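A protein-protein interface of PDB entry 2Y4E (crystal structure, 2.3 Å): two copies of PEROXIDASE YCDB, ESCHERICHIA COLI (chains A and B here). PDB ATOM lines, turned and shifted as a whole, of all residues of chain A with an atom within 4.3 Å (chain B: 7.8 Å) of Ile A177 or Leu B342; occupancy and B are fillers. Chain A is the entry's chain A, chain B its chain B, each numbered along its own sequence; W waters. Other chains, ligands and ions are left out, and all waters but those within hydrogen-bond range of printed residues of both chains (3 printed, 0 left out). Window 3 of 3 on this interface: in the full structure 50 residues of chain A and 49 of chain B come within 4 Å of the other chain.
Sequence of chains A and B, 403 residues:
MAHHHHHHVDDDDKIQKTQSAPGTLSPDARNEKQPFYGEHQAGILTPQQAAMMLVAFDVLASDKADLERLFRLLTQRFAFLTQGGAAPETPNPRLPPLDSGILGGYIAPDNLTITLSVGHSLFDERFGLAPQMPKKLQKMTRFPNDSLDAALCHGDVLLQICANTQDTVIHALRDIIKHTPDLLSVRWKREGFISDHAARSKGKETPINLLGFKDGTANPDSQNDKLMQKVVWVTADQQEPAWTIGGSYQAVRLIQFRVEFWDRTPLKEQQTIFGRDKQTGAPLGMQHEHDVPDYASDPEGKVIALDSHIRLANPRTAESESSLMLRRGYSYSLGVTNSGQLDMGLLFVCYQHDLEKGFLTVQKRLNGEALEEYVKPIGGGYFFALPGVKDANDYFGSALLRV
The guanidinium group of Arg A174 lies within salt-bridge range of the side-chain carboxylate of Asp B263, at 2.8 Å.
The side-chain amino group (NZ) of Lys A189 is in hydrogen-bond range of the side-chain hydroxyl (OG) of Ser B333 (3.2 Å).
NZ of Lys A189 lies within hydrogen-bond range of O of Leu B334, 2.7 Å away.
O of Gly B335 sits at hydrogen-bond distance from N of Asp B343.
The backbone NH (N) of Leu B342 lies within hydrogen-bond range of the side-chain carboxylate (OE2) of Glu B260, 2.8 Å away.
O of Asp B343 is in hydrogen-bond range of N of Leu B334.
Among the printed residues, merely in contact across the chains: Leu A173 with Leu B342 (3.8 Å), Arg A174 with Val B259 (3.5 Å), Ile A177 with Leu B342 (3.4 Å), Lys A178 with Asp B263 (3.9 Å), Val A186 with Val B336 (3.6 Å), Lys A189 with Gly B335 (3.5 Å) and Lys A189 with Leu B342 (3.8 Å).
Of chain B, only Leu B342 comes within 4 Å of Ile A177.
Of the printed residues of chain B, Lys A178 touches Asp B263.
Of the printed residues of chain A, Val B259 touches Arg A174.
Of the printed residues of chain A, Leu B334 touches Lys A189 (2.7 Å).
Printed residues of chain B within 4 Å of Val A186: Val B336 (3.6 Å).
Printed residues of chain A within 4 Å of Ser B333: Lys A189 (3.2 Å).
Phe B261 touches none of the printed residues of chain A.
The nearest printed residue of chain A that does not touch Leu B342 is Val A186 (4.3 Å).
Of the 21 printed residues of chain B, 7 touch a printed residue of chain A.
Printed residues of chain B that touch a printed residue of chain A: Val B259, Asp B263, Ser B333, Leu B334, Gly B335, Val B336 and Leu B342.
Of the 11 printed residues of chain A, 6 touch a printed residue of chain B.
Hydrophobic or aromatic side chains of chain A that line the printed part of chain B: Leu A173, Ile A177 and Val A186.
Among the printed residues, 10 pairs touch across the chains.
Among the printed residues, Asp or Glu carboxylates within 4 Å of a Lys or Arg side-chain nitrogen of the other chain: Arg A174 with Asp B263.
No position is printed for both chains.
Water W1 lies within hydrogen-bond range of the side-chain amino group of Lys A189 (2.4 Å), the backbone carbonyl oxygen of Gly B335 (2.8 Å), the backbone carbonyl oxygen of Asp B343 (2.8 Å) and the side-chain hydroxyl of Ser B333 (3.5 Å).
Water W3 lies within hydrogen-bond range of the side-chain carboxylate of Asp B263 and the backbone carbonyl oxygen of Arg A174.
Water W2 lies within hydrogen-bond range of the backbone carbonyl oxygen of Val A186 and the backbone carbonyl oxygen of Gly B340.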
ATOM      1  N   LEU A 173     -24.240  18.756  12.698  1.00  0.00           N
ATOM      2  CA  LEU A 173     -24.982  17.604  12.206  1.00  0.00           C
ATOM      3  C   LEU A 173     -24.158  16.327  12.185  1.00  0.00           C
ATOM      4  O   LEU A 173     -24.584  15.293  12.694  1.00  0.00           O
ATOM      5  CB  LEU A 173     -25.506  17.859  10.783  1.00  0.00           C
ATOM      6  CG  LEU A 173     -26.317  16.712  10.196  1.00  0.00           C
ATOM      7  CD1 LEU A 173     -27.468  16.337  11.139  1.00  0.00           C
ATOM      8  CD2 LEU A 173     -26.805  17.043   8.789  1.00  0.00           C
ATOM      9  N   ARG A 174     -22.982  16.407  11.585  1.00  0.00           N
ATOM     10  CA  ARG A 174     -22.147  15.220  11.423  1.00  0.00           C
ATOM     11  C   ARG A 174     -21.556  14.705  12.730  1.00  0.00           C
ATOM     12  O   ARG A 174     -21.331  13.483  12.889  1.00  0.00           O
ATOM     13  CB  ARG A 174     -21.103  15.440  10.335  1.00  0.00           C
ATOM     14  CG  ARG A 174     -21.730  15.139   8.976  1.00  0.00           C
ATOM     15  CD  ARG A 174     -20.853  15.453   7.826  1.00  0.00           C
ATOM     16  NE  ARG A 174     -19.612  14.688   7.809  1.00  0.00           N
ATOM     17  CZ  ARG A 174     -18.641  14.945   6.948  1.00  0.00           C
ATOM     18  NH1 ARG A 174     -18.836  15.900   6.041  1.00  0.00           N
ATOM     19  NH2 ARG A 174     -17.497  14.260   6.973  1.00  0.00           N
ATOM     20  N   ASP A 175     -21.366  15.622  13.677  1.00  0.00           N
ATOM     21  CA  ASP A 175     -20.981  15.255  15.031  1.00  0.00           C
ATOM     22  C   ASP A 175     -22.109  14.517  15.727  1.00  0.00           C
ATOM     23  O   ASP A 175     -21.886  13.490  16.359  1.00  0.00           O
ATOM     24  CB  ASP A 175     -20.598  16.514  15.837  1.00  0.00           C
ATOM     25  CG  ASP A 175     -20.202  16.205  17.259  1.00  0.00           C
ATOM     26  OD1 ASP A 175     -21.096  15.937  18.082  1.00  0.00           O
ATOM     27  OD2 ASP A 175     -18.998  16.269  17.569  1.00  0.00           O
ATOM     28  N   ILE A 176     -23.315  15.055  15.622  1.00  0.00           N
ATOM     29  CA  ILE A 176     -24.481  14.408  16.192  1.00  0.00           C
ATOM     30  C   ILE A 176     -24.710  13.025  15.557  1.00  0.00           C
ATOM     31  O   ILE A 176     -24.953  12.067  16.271  1.00  0.00           O
ATOM     32  CB  ILE A 176     -25.727  15.272  16.045  1.00  0.00           C
ATOM     33  CG1 ILE A 176     -25.581  16.541  16.884  1.00  0.00           C
ATOM     34  CG2 ILE A 176     -26.979  14.488  16.459  1.00  0.00           C
ATOM     35  CD1 ILE A 176     -26.312  17.745  16.308  1.00  0.00           C
ATOM     36  N   ILE A 177     -24.583  12.923  14.236  1.00  0.00           N
ATOM     37  CA  ILE A 177     -24.767  11.645  13.548  1.00  0.00           C
ATOM     38  C   ILE A 177     -23.726  10.612  13.945  1.00  0.00           C
ATOM     39  O   ILE A 177     -24.069   9.453  14.207  1.00  0.00           O
ATOM     40  CB  ILE A 177     -24.771  11.807  12.000  1.00  0.00           C
ATOM     41  CG1 ILE A 177     -26.074  12.474  11.558  1.00  0.00           C
ATOM     42  CG2 ILE A 177     -24.644  10.461  11.309  1.00  0.00           C
ATOM     43  CD1 ILE A 177     -26.145  12.757  10.063  1.00  0.00           C
ATOM     44  N   LYS A 178     -22.460  11.029  13.977  1.00  0.00           N
ATOM     45  CA  LYS A 178     -21.374  10.124  14.343  1.00  0.00           C
ATOM     46  C   LYS A 178     -21.657   9.486  15.703  1.00  0.00           C
ATOM     47  O   LYS A 178     -21.328   8.320  15.946  1.00  0.00           O
ATOM     48  CB  LYS A 178     -20.044  10.882  14.427  1.00  0.00           C
ATOM     49  CG  LYS A 178     -18.852   9.956  14.593  1.00  0.00           C
ATOM     50  CD  LYS A 178     -17.746  10.579  15.404  1.00  0.00           C
ATOM     51  CE  LYS A 178     -16.957   9.493  16.181  1.00  0.00           C
ATOM     52  NZ  LYS A 178     -16.046   8.677  15.345  1.00  0.00           N
ATOM     53  N   HIS A 179     -22.229  10.263  16.607  1.00  0.00           N
ATOM     54  CA  HIS A 179     -22.387   9.777  17.972  1.00  0.00           C
ATOM     55  C   HIS A 179     -23.666   8.990  18.221  1.00  0.00           C
ATOM     56  O   HIS A 179     -23.891   8.576  19.344  1.00  0.00           O
ATOM     57  CB  HIS A 179     -22.338  10.934  18.971  1.00  0.00           C
ATOM     58  CG  HIS A 179     -20.960  11.384  19.308  1.00  0.00           C
ATOM     59  ND1 HIS A 179     -20.377  12.486  18.718  1.00  0.00           N
ATOM     60  CD2 HIS A 179     -20.048  10.891  20.180  1.00  0.00           C
ATOM     61  CE1 HIS A 179     -19.157  12.645  19.205  1.00  0.00           C
ATOM     62  NE2 HIS A 179     -18.936  11.696  20.098  1.00  0.00           N
ATOM     63  N   THR A 180     -24.526   8.815  17.222  1.00  0.00           N
ATOM     64  CA  THR A 180     -25.854   8.210  17.497  1.00  0.00           C
ATOM     65  C   THR A 180     -26.299   7.183  16.449  1.00  0.00           C
ATOM     66  O   THR A 180     -27.481   7.133  16.104  1.00  0.00           O
ATOM     67  CB  THR A 180     -26.966   9.297  17.602  1.00  0.00           C
ATOM     68  OG1 THR A 180     -27.059   9.990  16.359  1.00  0.00           O
ATOM     69  CG2 THR A 180     -26.692  10.288  18.708  1.00  0.00           C
ATOM     70  N   PRO A 181     -25.368   6.345  15.946  1.00  0.00           N
ATOM     71  CA  PRO A 181     -25.755   5.447  14.826  1.00  0.00           C
ATOM     72  C   PRO A 181     -26.794   4.389  15.217  1.00  0.00           C
ATOM     73  O   PRO A 181     -27.562   3.910  14.364  1.00  0.00           O
ATOM     74  CB  PRO A 181     -24.436   4.789  14.423  1.00  0.00           C
ATOM     75  CG  PRO A 181     -23.558   4.859  15.672  1.00  0.00           C
ATOM     76  CD  PRO A 181     -24.041   6.015  16.511  1.00  0.00           C
ATOM     77  N   VAL A 186     -31.569   9.854  10.042  1.00  0.00           N
ATOM     78  CA  VAL A 186     -32.027  11.029   9.324  1.00  0.00           C
ATOM     79  C   VAL A 186     -33.260  10.679   8.514  1.00  0.00           C
ATOM     80  O   VAL A 186     -33.260   9.682   7.790  1.00  0.00           O
ATOM     81  CB  VAL A 186     -30.919  11.562   8.371  1.00  0.00           C
ATOM     82  CG1 VAL A 186     -31.426  12.736   7.533  1.00  0.00           C
ATOM     83  CG2 VAL A 186     -29.694  12.002   9.168  1.00  0.00           C
ATOM     84  N   LYS A 189     -34.123  16.551   5.547  1.00  0.00           N
ATOM     85  CA  LYS A 189     -33.232  17.658   5.871  1.00  0.00           C
ATOM     86  C   LYS A 189     -33.323  18.745   4.800  1.00  0.00           C
ATOM     87  O   LYS A 189     -33.306  18.434   3.589  1.00  0.00           O
ATOM     88  CB  LYS A 189     -31.793  17.172   5.954  1.00  0.00           C
ATOM     89  CG  LYS A 189     -30.738  18.316   5.713  1.00  0.00           C
ATOM     90  CD  LYS A 189     -29.330  17.827   5.945  1.00  0.00           C
ATOM     91  CE  LYS A 189     -28.299  18.822   5.483  1.00  0.00           C
ATOM     92  NZ  LYS A 189     -28.141  18.752   4.010  1.00  0.00           N
ATOM     93  N   GLN B 256     -21.019  12.879  -5.217  1.00  0.00           N
ATOM     94  CA  GLN B 256     -21.571  12.574  -3.889  1.00  0.00           C
ATOM     95  C   GLN B 256     -20.501  11.960  -2.994  1.00  0.00           C
ATOM     96  O   GLN B 256     -19.688  11.170  -3.464  1.00  0.00           O
ATOM     97  CB  GLN B 256     -22.781  11.622  -3.983  1.00  0.00           C
ATOM     98  CG  GLN B 256     -24.112  12.298  -3.701  1.00  0.00           C
ATOM     99  CD  GLN B 256     -25.338  11.545  -4.200  1.00  0.00           C
ATOM    100  OE1 GLN B 256     -25.370  10.329  -4.242  1.00  0.00           O
ATOM    101  NE2 GLN B 256     -26.362  12.290  -4.571  1.00  0.00           N
ATOM    102  N   PHE B 257     -20.502  12.329  -1.715  1.00  0.00           N
ATOM    103  CA  PHE B 257     -19.654  11.672  -0.723  1.00  0.00           C
ATOM    104  C   PHE B 257     -20.497  10.769   0.169  1.00  0.00           C
ATOM    105  O   PHE B 257     -21.589  11.163   0.599  1.00  0.00           O
ATOM    106  CB  PHE B 257     -18.974  12.700   0.189  1.00  0.00           C
ATOM    107  CG  PHE B 257     -17.991  13.592  -0.500  1.00  0.00           C
ATOM    108  CD1 PHE B 257     -17.472  13.263  -1.756  1.00  0.00           C
ATOM    109  CD2 PHE B 257     -17.551  14.753   0.129  1.00  0.00           C
ATOM    110  CE1 PHE B 257     -16.554  14.082  -2.382  1.00  0.00           C
ATOM    111  CE2 PHE B 257     -16.622  15.591  -0.502  1.00  0.00           C
ATOM    112  CZ  PHE B 257     -16.125  15.258  -1.763  1.00  0.00           C
ATOM    113  N   ARG B 258     -19.982   9.583   0.488  1.00  0.00           N
ATOM    114  CA  ARG B 258     -20.655   8.715   1.471  1.00  0.00           C
ATOM    115  C   ARG B 258     -20.182   9.152   2.868  1.00  0.00           C
ATOM    116  O   ARG B 258     -19.268   8.564   3.476  1.00  0.00           O
ATOM    117  CB  ARG B 258     -20.392   7.220   1.226  1.00  0.00           C
ATOM    118  CG  ARG B 258     -20.656   6.694  -0.189  1.00  0.00           C
ATOM    119  CD  ARG B 258     -21.326   5.311  -0.102  1.00  0.00           C
ATOM    120  NE  ARG B 258     -22.701   5.454   0.439  1.00  0.00           N
ATOM    121  CZ  ARG B 258     -23.154   4.941   1.592  1.00  0.00           C
ATOM    122  NH1 ARG B 258     -22.387   4.187   2.370  1.00  0.00           N
ATOM    123  NH2 ARG B 258     -24.398   5.169   1.960  1.00  0.00           N
ATOM    124  N   VAL B 259     -20.840  10.197   3.352  1.00  0.00           N
ATOM    125  CA  VAL B 259     -20.368  10.966   4.496  1.00  0.00           C
ATOM    126  C   VAL B 259     -20.435  10.227   5.828  1.00  0.00           C
ATOM    127  O   VAL B 259     -19.453  10.192   6.561  1.00  0.00           O
ATOM    128  CB  VAL B 259     -21.074  12.360   4.481  1.00  0.00           C
ATOM    129  CG1 VAL B 259     -21.663  12.727   5.807  1.00  0.00           C
ATOM    130  CG2 VAL B 259     -20.128  13.433   3.906  1.00  0.00           C
ATOM    131  N   GLU B 260     -21.566   9.605   6.128  1.00  0.00           N
ATOM    132  CA  GLU B 260     -21.720   8.871   7.387  1.00  0.00           C
ATOM    133  C   GLU B 260     -20.630   7.790   7.495  1.00  0.00           C
ATOM    134  O   GLU B 260     -19.926   7.679   8.507  1.00  0.00           O
ATOM    135  CB  GLU B 260     -23.099   8.237   7.463  1.00  0.00           C
ATOM    136  CG  GLU B 260     -24.252   9.236   7.474  1.00  0.00           C
ATOM    137  CD  GLU B 260     -24.830   9.529   6.079  1.00  0.00           C
ATOM    138  OE1 GLU B 260     -24.163   9.241   5.048  1.00  0.00           O
ATOM    139  OE2 GLU B 260     -25.973  10.037   6.029  1.00  0.00           O
ATOM    140  N   PHE B 261     -20.488   7.042   6.403  1.00  0.00           N
ATOM    141  CA  PHE B 261     -19.598   5.904   6.276  1.00  0.00           C
ATOM    142  C   PHE B 261     -18.142   6.348   6.396  1.00  0.00           C
ATOM    143  O   PHE B 261     -17.330   5.717   7.085  1.00  0.00           O
ATOM    144  CB  PHE B 261     -19.889   5.263   4.908  1.00  0.00           C
ATOM    145  CG  PHE B 261     -19.121   4.001   4.624  1.00  0.00           C
ATOM    146  CD1 PHE B 261     -19.057   2.969   5.553  1.00  0.00           C
ATOM    147  CD2 PHE B 261     -18.510   3.822   3.390  1.00  0.00           C
ATOM    148  CE1 PHE B 261     -18.349   1.781   5.257  1.00  0.00           C
ATOM    149  CE2 PHE B 261     -17.818   2.649   3.091  1.00  0.00           C
ATOM    150  CZ  PHE B 261     -17.732   1.637   4.034  1.00  0.00           C
ATOM    151  N   ASP B 263     -17.149   8.935   8.048  1.00  0.00           N
ATOM    152  CA  ASP B 263     -16.868   9.391   9.413  1.00  0.00           C
ATOM    153  C   ASP B 263     -16.732   8.195  10.345  1.00  0.00           C
ATOM    154  O   ASP B 263     -16.301   8.329  11.488  1.00  0.00           O
ATOM    155  CB  ASP B 263     -17.967  10.346   9.910  1.00  0.00           C
ATOM    156  CG  ASP B 263     -17.901  11.705   9.246  1.00  0.00           C
ATOM    157  OD1 ASP B 263     -16.929  12.000   8.512  1.00  0.00           O
ATOM    158  OD2 ASP B 263     -18.837  12.491   9.457  1.00  0.00           O
ATOM    159  N   ARG B 264     -17.109   7.026   9.829  1.00  0.00           N
ATOM    160  CA  ARG B 264     -16.932   5.776  10.538  1.00  0.00           C
ATOM    161  C   ARG B 264     -15.655   5.061  10.122  1.00  0.00           C
ATOM    162  O   ARG B 264     -15.395   3.933  10.560  1.00  0.00           O
ATOM    163  CB  ARG B 264     -18.117   4.861  10.299  1.00  0.00           C
ATOM    164  CG  ARG B 264     -19.359   5.252  11.052  1.00  0.00           C
ATOM    165  CD  ARG B 264     -20.382   4.185  10.887  1.00  0.00           C
ATOM    166  NE  ARG B 264     -21.655   4.777  10.501  1.00  0.00           N
ATOM    167  CZ  ARG B 264     -22.294   4.532   9.356  1.00  0.00           C
ATOM    168  NH1 ARG B 264     -21.818   3.669   8.451  1.00  0.00           N
ATOM    169  NH2 ARG B 264     -23.436   5.154   9.132  1.00  0.00           N
ATOM    170  N   TYR B 332     -20.763  21.103  -1.575  1.00  0.00           N
ATOM    171  CA  TYR B 332     -22.215  21.308  -1.617  1.00  0.00           C
ATOM    172  C   TYR B 332     -22.910  20.444  -0.591  1.00  0.00           C
ATOM    173  O   TYR B 332     -22.456  19.368  -0.244  1.00  0.00           O
ATOM    174  CB  TYR B 332     -22.812  21.049  -3.013  1.00  0.00           C
ATOM    175  CG  TYR B 332     -23.126  19.595  -3.269  1.00  0.00           C
ATOM    176  CD1 TYR B 332     -24.269  19.008  -2.730  1.00  0.00           C
ATOM    177  CD2 TYR B 332     -22.285  18.809  -4.044  1.00  0.00           C
ATOM    178  CE1 TYR B 332     -24.558  17.692  -2.923  1.00  0.00           C
ATOM    179  CE2 TYR B 332     -22.568  17.481  -4.259  1.00  0.00           C
ATOM    180  CZ  TYR B 332     -23.724  16.932  -3.690  1.00  0.00           C
ATOM    181  OH  TYR B 332     -24.036  15.621  -3.879  1.00  0.00           O
ATOM    182  N   SER B 333     -24.053  20.921  -0.143  1.00  0.00           N
ATOM    183  CA  SER B 333     -24.861  20.209   0.784  1.00  0.00           C
ATOM    184  C   SER B 333     -26.324  20.469   0.443  1.00  0.00           C
ATOM    185  O   SER B 333     -26.756  21.627   0.374  1.00  0.00           O
ATOM    186  CB  SER B 333     -24.552  20.685   2.207  1.00  0.00           C
ATOM    187  OG  SER B 333     -25.257  19.891   3.143  1.00  0.00           O
ATOM    188  N   LEU B 334     -27.085  19.399   0.226  1.00  0.00           N
ATOM    189  CA  LEU B 334     -28.461  19.526  -0.248  1.00  0.00           C
ATOM    190  C   LEU B 334     -29.390  18.943   0.790  1.00  0.00           C
ATOM    191  O   LEU B 334     -29.551  19.518   1.860  1.00  0.00           O
ATOM    192  CB  LEU B 334     -28.643  18.776  -1.568  1.00  0.00           C
ATOM    193  CG  LEU B 334     -28.240  19.528  -2.826  1.00  0.00           C
ATOM    194  CD1 LEU B 334     -28.033  18.563  -3.976  1.00  0.00           C
ATOM    195  CD2 LEU B 334     -29.291  20.584  -3.182  1.00  0.00           C
ATOM    196  N   GLY B 335     -29.982  17.782   0.491  1.00  0.00           N
ATOM    197  CA  GLY B 335     -30.852  17.117   1.453  1.00  0.00           C
ATOM    198  C   GLY B 335     -30.417  15.701   1.745  1.00  0.00           C
ATOM    199  O   GLY B 335     -29.324  15.454   2.255  1.00  0.00           O
ATOM    200  N   VAL B 336     -31.291  14.773   1.408  1.00  0.00           N
ATOM    201  CA  VAL B 336     -31.071  13.366   1.635  1.00  0.00           C
ATOM    202  C   VAL B 336     -30.974  12.725   0.245  1.00  0.00           C
ATOM    203  O   VAL B 336     -31.443  13.328  -0.747  1.00  0.00           O
ATOM    204  CB  VAL B 336     -32.226  12.813   2.524  1.00  0.00           C
ATOM    205  CG1 VAL B 336     -32.435  11.381   2.339  1.00  0.00           C
ATOM    206  CG2 VAL B 336     -31.938  13.109   3.994  1.00  0.00           C
ATOM    207  N   THR B 337     -30.326  11.559   0.150  1.00  0.00           N
ATOM    208  CA  THR B 337     -30.261  10.807  -1.119  1.00  0.00           C
ATOM    209  C   THR B 337     -31.437   9.859  -1.179  1.00  0.00           C
ATOM    210  O   THR B 337     -32.155   9.683  -0.178  1.00  0.00           O
ATOM    211  CB  THR B 337     -28.975   9.963  -1.269  1.00  0.00           C
ATOM    212  OG1 THR B 337     -29.016   8.870  -0.342  1.00  0.00           O
ATOM    213  CG2 THR B 337     -27.733  10.820  -0.995  1.00  0.00           C
ATOM    214  N   SER B 339     -31.501   6.757  -1.068  1.00  0.00           N
ATOM    215  CA  SER B 339     -31.412   5.701  -0.060  1.00  0.00           C
ATOM    216  C   SER B 339     -31.442   6.191   1.390  1.00  0.00           C
ATOM    217  O   SER B 339     -31.281   5.401   2.296  1.00  0.00           O
ATOM    218  CB  SER B 339     -30.169   4.837  -0.302  1.00  0.00           C
ATOM    219  OG  SER B 339     -29.060   5.621  -0.696  1.00  0.00           O
ATOM    220  N   GLY B 340     -31.641   7.483   1.630  1.00  0.00           N
ATOM    221  CA  GLY B 340     -31.737   7.974   3.001  1.00  0.00           C
ATOM    222  C   GLY B 340     -30.490   8.592   3.633  1.00  0.00           C
ATOM    223  O   GLY B 340     -30.554   9.085   4.752  1.00  0.00           O
ATOM    224  N   GLN B 341     -29.355   8.564   2.947  1.00  0.00           N
ATOM    225  CA  GLN B 341     -28.150   9.158   3.500  1.00  0.00           C
ATOM    226  C   GLN B 341     -28.049  10.639   3.160  1.00  0.00           C
ATOM    227  O   GLN B 341     -28.763  11.117   2.296  1.00  0.00           O
ATOM    228  CB  GLN B 341     -26.908   8.425   3.006  1.00  0.00           C
ATOM    229  CG  GLN B 341     -26.602   7.180   3.806  1.00  0.00           C
ATOM    230  CD  GLN B 341     -27.652   6.151   3.590  1.00  0.00           C
ATOM    231  OE1 GLN B 341     -27.813   5.649   2.467  1.00  0.00           O
ATOM    232  NE2 GLN B 341     -28.428   5.857   4.644  1.00  0.00           N
ATOM    233  N   LEU B 342     -27.181  11.360   3.861  1.00  0.00           N
ATOM    234  CA  LEU B 342     -26.954  12.786   3.597  1.00  0.00           C
ATOM    235  C   LEU B 342     -26.438  12.991   2.178  1.00  0.00           C
ATOM    236  O   LEU B 342     -25.505  12.331   1.752  1.00  0.00           O
ATOM    237  CB  LEU B 342     -25.957  13.363   4.607  1.00  0.00           C
ATOM    238  CG  LEU B 342     -26.457  13.466   6.050  1.00  0.00           C
ATOM    239  CD1 LEU B 342     -25.350  13.985   6.964  1.00  0.00           C
ATOM    240  CD2 LEU B 342     -27.720  14.393   6.150  1.00  0.00           C
ATOM    241  N   ASP B 343     -27.069  13.897   1.453  1.00  0.00           N
ATOM    242  CA  ASP B 343     -26.642  14.253   0.117  1.00  0.00           C
ATOM    243  C   ASP B 343     -25.665  15.428   0.197  1.00  0.00           C
ATOM    244  O   ASP B 343     -26.068  16.588   0.352  1.00  0.00           O
ATOM    245  CB  ASP B 343     -27.863  14.597  -0.738  1.00  0.00           C
ATOM    246  CG  ASP B 343     -27.521  14.866  -2.199  1.00  0.00           C
ATOM    247  OD1 ASP B 343     -26.335  14.750  -2.615  1.00  0.00           O
ATOM    248  OD2 ASP B 343     -28.472  15.184  -2.952  1.00  0.00           O
ATOM    249  N   MET B 344     -24.379  15.122   0.127  1.00  0.00           N
ATOM    250  CA  MET B 344     -23.384  16.174   0.120  1.00  0.00           C
ATOM    251  C   MET B 344     -22.097  15.709  -0.536  1.00  0.00           C
ATOM    252  O   MET B 344     -21.820  14.488  -0.626  1.00  0.00           O
ATOM    253  CB  MET B 344     -23.145  16.785   1.524  1.00  0.00           C
ATOM    254  CG  MET B 344     -22.731  15.832   2.622  1.00  0.00           C
ATOM    255  SD  MET B 344     -22.406  16.596   4.259  1.00  0.00           S
ATOM    256  CE  MET B 344     -24.036  17.062   4.844  1.00  0.00           C
ATOM    257  N   GLY B 345     -21.349  16.672  -1.056  1.00  0.00           N
ATOM    258  CA  GLY B 345     -20.019  16.374  -1.568  1.00  0.00           C
ATOM    259  C   GLY B 345     -19.356  17.536  -2.253  1.00  0.00           C
ATOM    260  O   GLY B 345     -19.271  18.635  -1.710  1.00  0.00           O
HETATM  261  O   HOH W   1     -27.001  16.865   3.011  1.00  0.00           O
HETATM  262  O   HOH W   2     -31.597   7.809   6.883  1.00  0.00           O
HETATM  263  O   HOH W   3     -21.016  11.757  10.676  1.00  0.00           O
